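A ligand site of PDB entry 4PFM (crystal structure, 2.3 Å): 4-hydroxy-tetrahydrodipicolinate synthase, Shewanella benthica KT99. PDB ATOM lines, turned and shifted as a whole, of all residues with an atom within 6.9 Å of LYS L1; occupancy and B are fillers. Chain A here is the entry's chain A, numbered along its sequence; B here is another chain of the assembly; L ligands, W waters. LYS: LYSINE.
OH of Tyr 107 of chain A sits at hydrogen-bond distance from O of LYS L1 (2.5 Å).
O of Ala 50 sits at hydrogen-bond distance from N of LYS L1 (2.6 Å).
A nitrogen (N) of LYS L1 sits at hydrogen-bond distance from the side-chain amide oxygen (OD1) of Asn 81 of chain B.
A nitrogen (NZ) of LYS L1 is in hydrogen-bond range of the backbone carbonyl oxygen of Leu 52.
ND1 of His 57 sits at hydrogen-bond distance from NZ of LYS L1.
The backbone carbonyl oxygen (O) of Ser 49 sits at hydrogen-bond distance from a nitrogen (NZ) of LYS L1 (2.9 Å).
OE1 of Glu 85 of chain B lies within salt-bridge range of N of LYS L1.
OD1 of Asn 81 of chain A sits at hydrogen-bond distance from N of LYS L2.
The side-chain carboxylate of Glu 85 of chain A is in salt-bridge range of a nitrogen (N) of LYS L2 (2.7 Å).
An oxygen (O) of LYS L2 lies within hydrogen-bond range of the side-chain hydroxyl of Tyr 107 of chain B (2.6 Å).
O of Tyr 107 of chain A lies within hydrogen-bond range of ND2 of Asn 81 of chain A (3.2 Å).
The side-chain amide nitrogen of Asn 81 of chain B sits at hydrogen-bond distance from the backbone carbonyl oxygen of Tyr 107 of chain B (3.1 Å).
The backbone carbonyl oxygen (O) of Asn 81 of chain B sits at hydrogen-bond distance from the side-chain amide nitrogen (ND2) of Asn 109 of chain B, 3.0 Å away.
Of the 24 residues printed, 7 come within 4 Å of LYS L1.
The nearest printed residue that does not touch LYS L1 is Ala 82 of chain B (4.2 Å).
Water W1 lies within hydrogen-bond range of O of LYS L1 (2.7 Å), OE1 of Glu 85 of chain A (2.8 Å) and OH of Tyr 107 of chain A (3.1 Å).
Water W2 lies within hydrogen-bond range of an oxygen (OXT) of LYS L1 (2.8 Å), the side-chain hydroxyl of Ser 49 (3.0 Å), the side-chain hydroxyl of Tyr 107 of chain A (3.2 Å) and the backbone NH of Ala 50 (3.3 Å).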
ATOM      1  N   VAL A  43      26.076 -20.420 -25.597  1.00  0.00           N
ATOM      2  CA  VAL A  43      25.221 -20.766 -24.471  1.00  0.00           C
ATOM      3  C   VAL A  43      26.007 -20.775 -23.105  1.00  0.00           C
ATOM      4  O   VAL A  43      25.951 -21.741 -22.316  1.00  0.00           O
ATOM      5  CB  VAL A  43      24.436 -22.078 -24.731  1.00  0.00           C
ATOM      6  CG1 VAL A  43      23.242 -22.185 -23.844  1.00  0.00           C
ATOM      7  CG2 VAL A  43      24.065 -22.150 -26.218  1.00  0.00           C
ATOM      8  N   GLU A  48      22.145 -16.903 -22.323  1.00  0.00           N
ATOM      9  CA  GLU A  48      20.829 -17.244 -21.761  1.00  0.00           C
ATOM     10  C   GLU A  48      20.637 -18.780 -21.587  1.00  0.00           C
ATOM     11  O   GLU A  48      19.490 -19.308 -21.776  1.00  0.00           O
ATOM     12  CB  GLU A  48      19.658 -16.670 -22.617  1.00  0.00           C
ATOM     13  CG  GLU A  48      19.557 -15.152 -22.705  1.00  0.00           C
ATOM     14  CD  GLU A  48      18.375 -14.615 -23.649  1.00  0.00           C
ATOM     15  OE1 GLU A  48      17.159 -14.808 -23.359  1.00  0.00           O
ATOM     16  OE2 GLU A  48      18.674 -13.973 -24.703  1.00  0.00           O
ATOM     17  N   SER A  49      21.706 -19.466 -21.200  1.00  0.00           N
ATOM     18  CA  SER A  49      21.613 -20.894 -20.936  1.00  0.00           C
ATOM     19  C   SER A  49      20.390 -21.247 -20.127  1.00  0.00           C
ATOM     20  O   SER A  49      19.651 -22.160 -20.480  1.00  0.00           O
ATOM     21  CB  SER A  49      22.900 -21.370 -20.204  1.00  0.00           C
ATOM     22  OG  SER A  49      22.935 -20.761 -18.936  1.00  0.00           O
ATOM     23  N   ALA A  50      20.112 -20.500 -19.051  1.00  0.00           N
ATOM     24  CA  ALA A  50      18.964 -20.839 -18.217  1.00  0.00           C
ATOM     25  C   ALA A  50      17.622 -21.004 -18.938  1.00  0.00           C
ATOM     26  O   ALA A  50      16.772 -21.844 -18.508  1.00  0.00           O
ATOM     27  CB  ALA A  50      18.797 -19.825 -17.148  1.00  0.00           C
ATOM     28  N   THR A  51      17.376 -20.244 -20.020  1.00  0.00           N
ATOM     29  CA  THR A  51      16.045 -20.334 -20.608  1.00  0.00           C
ATOM     30  C   THR A  51      16.004 -21.140 -21.893  1.00  0.00           C
ATOM     31  O   THR A  51      14.999 -21.109 -22.628  1.00  0.00           O
ATOM     32  CB  THR A  51      15.450 -18.938 -20.821  1.00  0.00           C
ATOM     33  OG1 THR A  51      16.364 -18.095 -21.558  1.00  0.00           O
ATOM     34  CG2 THR A  51      15.214 -18.330 -19.442  1.00  0.00           C
ATOM     35  N   LEU A  52      17.085 -21.861 -22.173  1.00  0.00           N
ATOM     36  CA  LEU A  52      17.122 -22.802 -23.316  1.00  0.00           C
ATOM     37  C   LEU A  52      16.996 -24.184 -22.736  1.00  0.00           C
ATOM     38  O   LEU A  52      17.896 -24.639 -22.003  1.00  0.00           O
ATOM     39  CB  LEU A  52      18.431 -22.669 -24.135  1.00  0.00           C
ATOM     40  CG  LEU A  52      18.647 -21.283 -24.825  1.00  0.00           C
ATOM     41  CD1 LEU A  52      20.081 -21.054 -25.320  1.00  0.00           C
ATOM     42  CD2 LEU A  52      17.749 -21.290 -26.005  1.00  0.00           C
ATOM     43  N   PRO A  53      15.891 -24.865 -23.045  1.00  0.00           N
ATOM     44  CA  PRO A  53      15.855 -26.300 -22.591  1.00  0.00           C
ATOM     45  C   PRO A  53      16.970 -27.072 -23.276  1.00  0.00           C
ATOM     46  O   PRO A  53      17.511 -26.611 -24.312  1.00  0.00           O
ATOM     47  CB  PRO A  53      14.528 -26.831 -23.144  1.00  0.00           C
ATOM     48  CG  PRO A  53      13.940 -25.643 -24.047  1.00  0.00           C
ATOM     49  CD  PRO A  53      14.632 -24.388 -23.658  1.00  0.00           C
ATOM     50  N   ILE A  54      17.322 -28.233 -22.722  1.00  0.00           N
ATOM     51  CA  ILE A  54      18.452 -28.972 -23.263  1.00  0.00           C
ATOM     52  C   ILE A  54      18.463 -29.090 -24.796  1.00  0.00           C
ATOM     53  O   ILE A  54      19.456 -28.781 -25.418  1.00  0.00           O
ATOM     54  CB  ILE A  54      18.679 -30.358 -22.580  1.00  0.00           C
ATOM     55  CG1 ILE A  54      19.884 -31.032 -23.231  1.00  0.00           C
ATOM     56  CG2 ILE A  54      17.475 -31.309 -22.747  1.00  0.00           C
ATOM     57  CD1 ILE A  54      20.337 -32.259 -22.450  1.00  0.00           C
ATOM     58  N   SER A  55      17.356 -29.468 -25.417  1.00  0.00           N
ATOM     59  CA  SER A  55      17.385 -29.700 -26.865  1.00  0.00           C
ATOM     60  C   SER A  55      17.729 -28.417 -27.614  1.00  0.00           C
ATOM     61  O   SER A  55      18.458 -28.441 -28.553  1.00  0.00           O
ATOM     62  CB  SER A  55      16.017 -30.237 -27.372  1.00  0.00           C
ATOM     63  OG  SER A  55      14.981 -29.205 -27.240  1.00  0.00           O
ATOM     64  N   HIS A  57      19.398 -25.852 -26.321  1.00  0.00           N
ATOM     65  CA  HIS A  57      20.708 -25.462 -25.858  1.00  0.00           C
ATOM     66  C   HIS A  57      21.691 -26.174 -26.777  1.00  0.00           C
ATOM     67  O   HIS A  57      22.573 -25.565 -27.365  1.00  0.00           O
ATOM     68  CB  HIS A  57      20.851 -25.949 -24.416  1.00  0.00           C
ATOM     69  CG  HIS A  57      22.180 -25.732 -23.791  1.00  0.00           C
ATOM     70  ND1 HIS A  57      22.311 -25.332 -22.476  1.00  0.00           N
ATOM     71  CD2 HIS A  57      23.444 -25.894 -24.264  1.00  0.00           C
ATOM     72  CE1 HIS A  57      23.603 -25.296 -22.158  1.00  0.00           C
ATOM     73  NE2 HIS A  57      24.307 -25.602 -23.237  1.00  0.00           N
ATOM     74  N   GLY A  79      27.405 -25.908 -18.094  1.00  0.00           N
ATOM     75  CA  GLY A  79      27.194 -25.969 -16.617  1.00  0.00           C
ATOM     76  C   GLY A  79      25.783 -26.349 -16.230  1.00  0.00           C
ATOM     77  O   GLY A  79      24.851 -26.161 -16.983  1.00  0.00           O
ATOM     78  N   ALA A  80      25.637 -26.909 -15.063  1.00  0.00           N
ATOM     79  CA  ALA A  80      24.341 -27.256 -14.470  1.00  0.00           C
ATOM     80  C   ALA A  80      24.563 -27.249 -12.964  1.00  0.00           C
ATOM     81  O   ALA A  80      25.687 -27.339 -12.509  1.00  0.00           O
ATOM     82  CB  ALA A  80      23.937 -28.637 -14.900  1.00  0.00           C
ATOM     83  N   ASN A  81      23.509 -27.106 -12.202  1.00  0.00           N
ATOM     84  CA  ASN A  81      23.595 -27.241 -10.757  1.00  0.00           C
ATOM     85  C   ASN A  81      23.203 -28.614 -10.219  1.00  0.00           C
ATOM     86  O   ASN A  81      23.099 -28.797  -9.007  1.00  0.00           O
ATOM     87  CB  ASN A  81      22.770 -26.148 -10.061  1.00  0.00           C
ATOM     88  CG  ASN A  81      21.282 -26.251 -10.385  1.00  0.00           C
ATOM     89  OD1 ASN A  81      20.850 -27.116 -11.139  1.00  0.00           O
ATOM     90  ND2 ASN A  81      20.474 -25.332  -9.804  1.00  0.00           N
ATOM     91  N   ALA A  82      22.902 -29.549 -11.126  1.00  0.00           N
ATOM     92  CA  ALA A  82      22.796 -31.010 -10.860  1.00  0.00           C
ATOM     93  C   ALA A  82      23.882 -31.706 -11.637  1.00  0.00           C
ATOM     94  O   ALA A  82      23.976 -31.584 -12.915  1.00  0.00           O
ATOM     95  CB  ALA A  82      21.468 -31.577 -11.276  1.00  0.00           C
ATOM     96  N   GLU A  85      22.840 -33.435 -14.683  1.00  0.00           N
ATOM     97  CA  GLU A  85      22.376 -32.617 -15.825  1.00  0.00           C
ATOM     98  C   GLU A  85      23.591 -32.158 -16.553  1.00  0.00           C
ATOM     99  O   GLU A  85      23.585 -32.092 -17.729  1.00  0.00           O
ATOM    100  CB  GLU A  85      21.530 -31.405 -15.402  1.00  0.00           C
ATOM    101  CG  GLU A  85      20.082 -31.767 -15.203  1.00  0.00           C
ATOM    102  CD  GLU A  85      19.284 -30.693 -14.412  1.00  0.00           C
ATOM    103  OE1 GLU A  85      19.921 -29.750 -13.873  1.00  0.00           O
ATOM    104  OE2 GLU A  85      18.024 -30.821 -14.283  1.00  0.00           O
ATOM    105  N   LEU A  89      24.600 -32.825 -20.619  1.00  0.00           N
ATOM    106  CA  LEU A  89      24.907 -31.741 -21.566  1.00  0.00           C
ATOM    107  C   LEU A  89      26.286 -31.968 -22.208  1.00  0.00           C
ATOM    108  O   LEU A  89      26.488 -31.712 -23.419  1.00  0.00           O
ATOM    109  CB  LEU A  89      24.950 -30.451 -20.789  1.00  0.00           C
ATOM    110  CG  LEU A  89      24.212 -29.147 -20.987  1.00  0.00           C
ATOM    111  CD1 LEU A  89      22.919 -29.169 -21.792  1.00  0.00           C
ATOM    112  CD2 LEU A  89      23.974 -28.619 -19.618  1.00  0.00           C
ATOM    113  N   TYR A 107      24.751 -23.374  -9.242  1.00  0.00           N
ATOM    114  CA  TYR A 107      24.158 -22.198  -8.686  1.00  0.00           C
ATOM    115  C   TYR A 107      23.024 -22.570  -7.785  1.00  0.00           C
ATOM    116  O   TYR A 107      22.393 -23.615  -7.959  1.00  0.00           O
ATOM    117  CB  TYR A 107      23.640 -21.310  -9.848  1.00  0.00           C
ATOM    118  CG  TYR A 107      23.151 -22.078 -11.013  1.00  0.00           C
ATOM    119  CD1 TYR A 107      24.034 -22.438 -12.022  1.00  0.00           C
ATOM    120  CD2 TYR A 107      21.831 -22.473 -11.117  1.00  0.00           C
ATOM    121  CE1 TYR A 107      23.599 -23.213 -13.142  1.00  0.00           C
ATOM    122  CE2 TYR A 107      21.362 -23.227 -12.228  1.00  0.00           C
ATOM    123  CZ  TYR A 107      22.267 -23.590 -13.234  1.00  0.00           C
ATOM    124  OH  TYR A 107      21.905 -24.349 -14.343  1.00  0.00           O
ATOM    125  N   ALA B  80      11.279 -22.023 -10.778  1.00  0.00           N
ATOM    126  CA  ALA B  80      12.259 -22.318 -11.843  1.00  0.00           C
ATOM    127  C   ALA B  80      12.868 -20.975 -12.254  1.00  0.00           C
ATOM    128  O   ALA B  80      12.229 -19.870 -12.019  1.00  0.00           O
ATOM    129  CB  ALA B  80      11.573 -22.974 -13.049  1.00  0.00           C
ATOM    130  N   ASN B  81      14.048 -20.985 -12.829  1.00  0.00           N
ATOM    131  CA  ASN B  81      14.599 -19.733 -13.317  1.00  0.00           C
ATOM    132  C   ASN B  81      14.326 -19.420 -14.780  1.00  0.00           C
ATOM    133  O   ASN B  81      14.859 -18.472 -15.271  1.00  0.00           O
ATOM    134  CB  ASN B  81      16.080 -19.655 -13.051  1.00  0.00           C
ATOM    135  CG  ASN B  81      16.841 -20.695 -13.830  1.00  0.00           C
ATOM    136  OD1 ASN B  81      16.236 -21.509 -14.546  1.00  0.00           O
ATOM    137  ND2 ASN B  81      18.162 -20.701 -13.660  1.00  0.00           N
ATOM    138  N   ALA B  82      13.573 -20.286 -15.462  1.00  0.00           N
ATOM    139  CA  ALA B  82      13.003 -20.054 -16.746  1.00  0.00           C
ATOM    140  C   ALA B  82      11.490 -19.977 -16.618  1.00  0.00           C
ATOM    141  O   ALA B  82      10.849 -20.930 -16.187  1.00  0.00           O
ATOM    142  CB  ALA B  82      13.375 -21.267 -17.701  1.00  0.00           C
ATOM    143  N   GLU B  85       9.582 -23.022 -17.826  1.00  0.00           N
ATOM    144  CA  GLU B  85       9.863 -24.246 -17.097  1.00  0.00           C
ATOM    145  C   GLU B  85       8.997 -24.236 -15.855  1.00  0.00           C
ATOM    146  O   GLU B  85       8.415 -25.270 -15.487  1.00  0.00           O
ATOM    147  CB  GLU B  85      11.370 -24.289 -16.806  1.00  0.00           C
ATOM    148  CG  GLU B  85      11.999 -25.611 -16.459  1.00  0.00           C
ATOM    149  CD  GLU B  85      13.417 -25.441 -15.823  1.00  0.00           C
ATOM    150  OE1 GLU B  85      14.012 -24.319 -15.898  1.00  0.00           O
ATOM    151  OE2 GLU B  85      13.917 -26.447 -15.231  1.00  0.00           O
ATOM    152  N   TYR B 107      16.651 -17.898 -10.047  1.00  0.00           N
ATOM    153  CA  TYR B 107      17.991 -17.808  -9.512  1.00  0.00           C
ATOM    154  C   TYR B 107      19.004 -17.797 -10.644  1.00  0.00           C
ATOM    155  O   TYR B 107      18.700 -18.291 -11.717  1.00  0.00           O
ATOM    156  CB  TYR B 107      18.259 -18.993  -8.567  1.00  0.00           C
ATOM    157  CG  TYR B 107      17.595 -20.238  -9.057  1.00  0.00           C
ATOM    158  CD1 TYR B 107      18.213 -21.045 -10.008  1.00  0.00           C
ATOM    159  CD2 TYR B 107      16.349 -20.569  -8.635  1.00  0.00           C
ATOM    160  CE1 TYR B 107      17.564 -22.173 -10.532  1.00  0.00           C
ATOM    161  CE2 TYR B 107      15.691 -21.718  -9.129  1.00  0.00           C
ATOM    162  CZ  TYR B 107      16.316 -22.502 -10.074  1.00  0.00           C
ATOM    163  OH  TYR B 107      15.655 -23.635 -10.515  1.00  0.00           O
ATOM    164  N   TYR B 108      20.187 -17.187 -10.394  1.00  0.00           N
ATOM    165  CA  TYR B 108      21.347 -17.184 -11.270  1.00  0.00           C
ATOM    166  C   TYR B 108      21.211 -16.198 -12.455  1.00  0.00           C
ATOM    167  O   TYR B 108      22.184 -15.510 -12.835  1.00  0.00           O
ATOM    168  CB  TYR B 108      21.628 -18.626 -11.776  1.00  0.00           C
ATOM    169  CG  TYR B 108      22.702 -18.704 -12.832  1.00  0.00           C
ATOM    170  CD1 TYR B 108      24.046 -18.549 -12.484  1.00  0.00           C
ATOM    171  CD2 TYR B 108      22.394 -18.967 -14.169  1.00  0.00           C
ATOM    172  CE1 TYR B 108      25.027 -18.647 -13.416  1.00  0.00           C
ATOM    173  CE2 TYR B 108      23.388 -19.102 -15.135  1.00  0.00           C
ATOM    174  CZ  TYR B 108      24.703 -18.915 -14.735  1.00  0.00           C
ATOM    175  OH  TYR B 108      25.749 -18.987 -15.638  1.00  0.00           O
ATOM    176  N   ASN B 109      20.015 -16.150 -13.084  1.00  0.00           N
ATOM    177  CA  ASN B 109      19.918 -15.164 -14.191  1.00  0.00           C
ATOM    178  C   ASN B 109      19.486 -13.736 -13.801  1.00  0.00           C
ATOM    179  O   ASN B 109      19.526 -12.848 -14.656  1.00  0.00           O
ATOM    180  CB  ASN B 109      19.166 -15.719 -15.390  1.00  0.00           C
ATOM    181  CG  ASN B 109      17.742 -16.133 -15.053  1.00  0.00           C
ATOM    182  OD1 ASN B 109      17.307 -16.048 -13.921  1.00  0.00           O
ATOM    183  ND2 ASN B 109      17.015 -16.602 -16.050  1.00  0.00           N
HETATM  184  N   LYS L   1      16.689 -23.459 -16.411  1.00  0.00           N
HETATM  185  CA  LYS L   1      17.420 -24.611 -15.804  1.00  0.00           C
HETATM  186  C   LYS L   1      18.777 -24.102 -15.193  1.00  0.00           C
HETATM  187  O   LYS L   1      19.472 -24.944 -14.627  1.00  0.00           O
HETATM  188  CB  LYS L   1      17.633 -25.728 -16.839  1.00  0.00           C
HETATM  189  CG  LYS L   1      18.553 -25.349 -18.059  1.00  0.00           C
HETATM  190  CD  LYS L   1      18.679 -26.483 -19.118  1.00  0.00           C
HETATM  191  CE  LYS L   1      19.893 -26.321 -19.999  1.00  0.00           C
HETATM  192  NZ  LYS L   1      20.234 -24.955 -20.582  1.00  0.00           N
HETATM  193  OXT LYS L   1      19.211 -22.903 -15.240  1.00  0.00           O
HETATM  194  N   LYS L   2      18.707 -28.332 -11.949  1.00  0.00           N
HETATM  195  CA  LYS L   2      17.750 -27.432 -12.666  1.00  0.00           C
HETATM  196  C   LYS L   2      17.313 -26.210 -11.797  1.00  0.00           C
HETATM  197  O   LYS L   2      16.459 -25.429 -12.204  1.00  0.00           O
HETATM  198  CB  LYS L   2      16.509 -28.210 -13.166  1.00  0.00           C
HETATM  199  CG  LYS L   2      15.384 -28.449 -12.128  1.00  0.00           C
HETATM  200  CD  LYS L   2      14.315 -29.485 -12.581  1.00  0.00           C
HETATM  201  CE  LYS L   2      13.041 -29.345 -11.721  1.00  0.00           C
HETATM  202  NZ  LYS L   2      13.218 -29.677 -10.279  1.00  0.00           N
HETATM  203  OXT LYS L   2      17.767 -26.014 -10.681  1.00  0.00           O
HETATM  204  N   LYS L   3      13.973 -23.789 -20.251  1.00  0.00           N
HETATM  205  CA  LYS L   3      12.748 -24.616 -19.918  1.00  0.00           C
HETATM  206  C   LYS L   3      13.228 -25.990 -19.406  1.00  0.00           C
HETATM  207  O   LYS L   3      12.555 -27.093 -19.413  1.00  0.00           O
HETATM  208  CB  LYS L   3      11.756 -24.747 -21.095  1.00  0.00           C
HETATM  209  CG  LYS L   3      10.395 -25.423 -20.772  1.00  0.00           C
HETATM  210  CD  LYS L   3      10.299 -26.942 -20.891  1.00  0.00           C
HETATM  211  CE  LYS L   3      10.454 -27.536 -22.373  1.00  0.00           C
HETATM  212  NZ  LYS L   3       9.818 -28.891 -22.453  1.00  0.00           N
HETATM  213  OXT LYS L   3      14.387 -25.926 -18.951  1.00  0.00           O
HETATM  214  O   HOH W   1      20.865 -27.215 -14.677  1.00  0.00           O
HETATM  215  O   HOH W   2      21.597 -22.109 -16.575  1.00  0.00           O
HETATM  216  O   HOH W   3      21.881 -26.438 -17.228  1.00  0.00           O
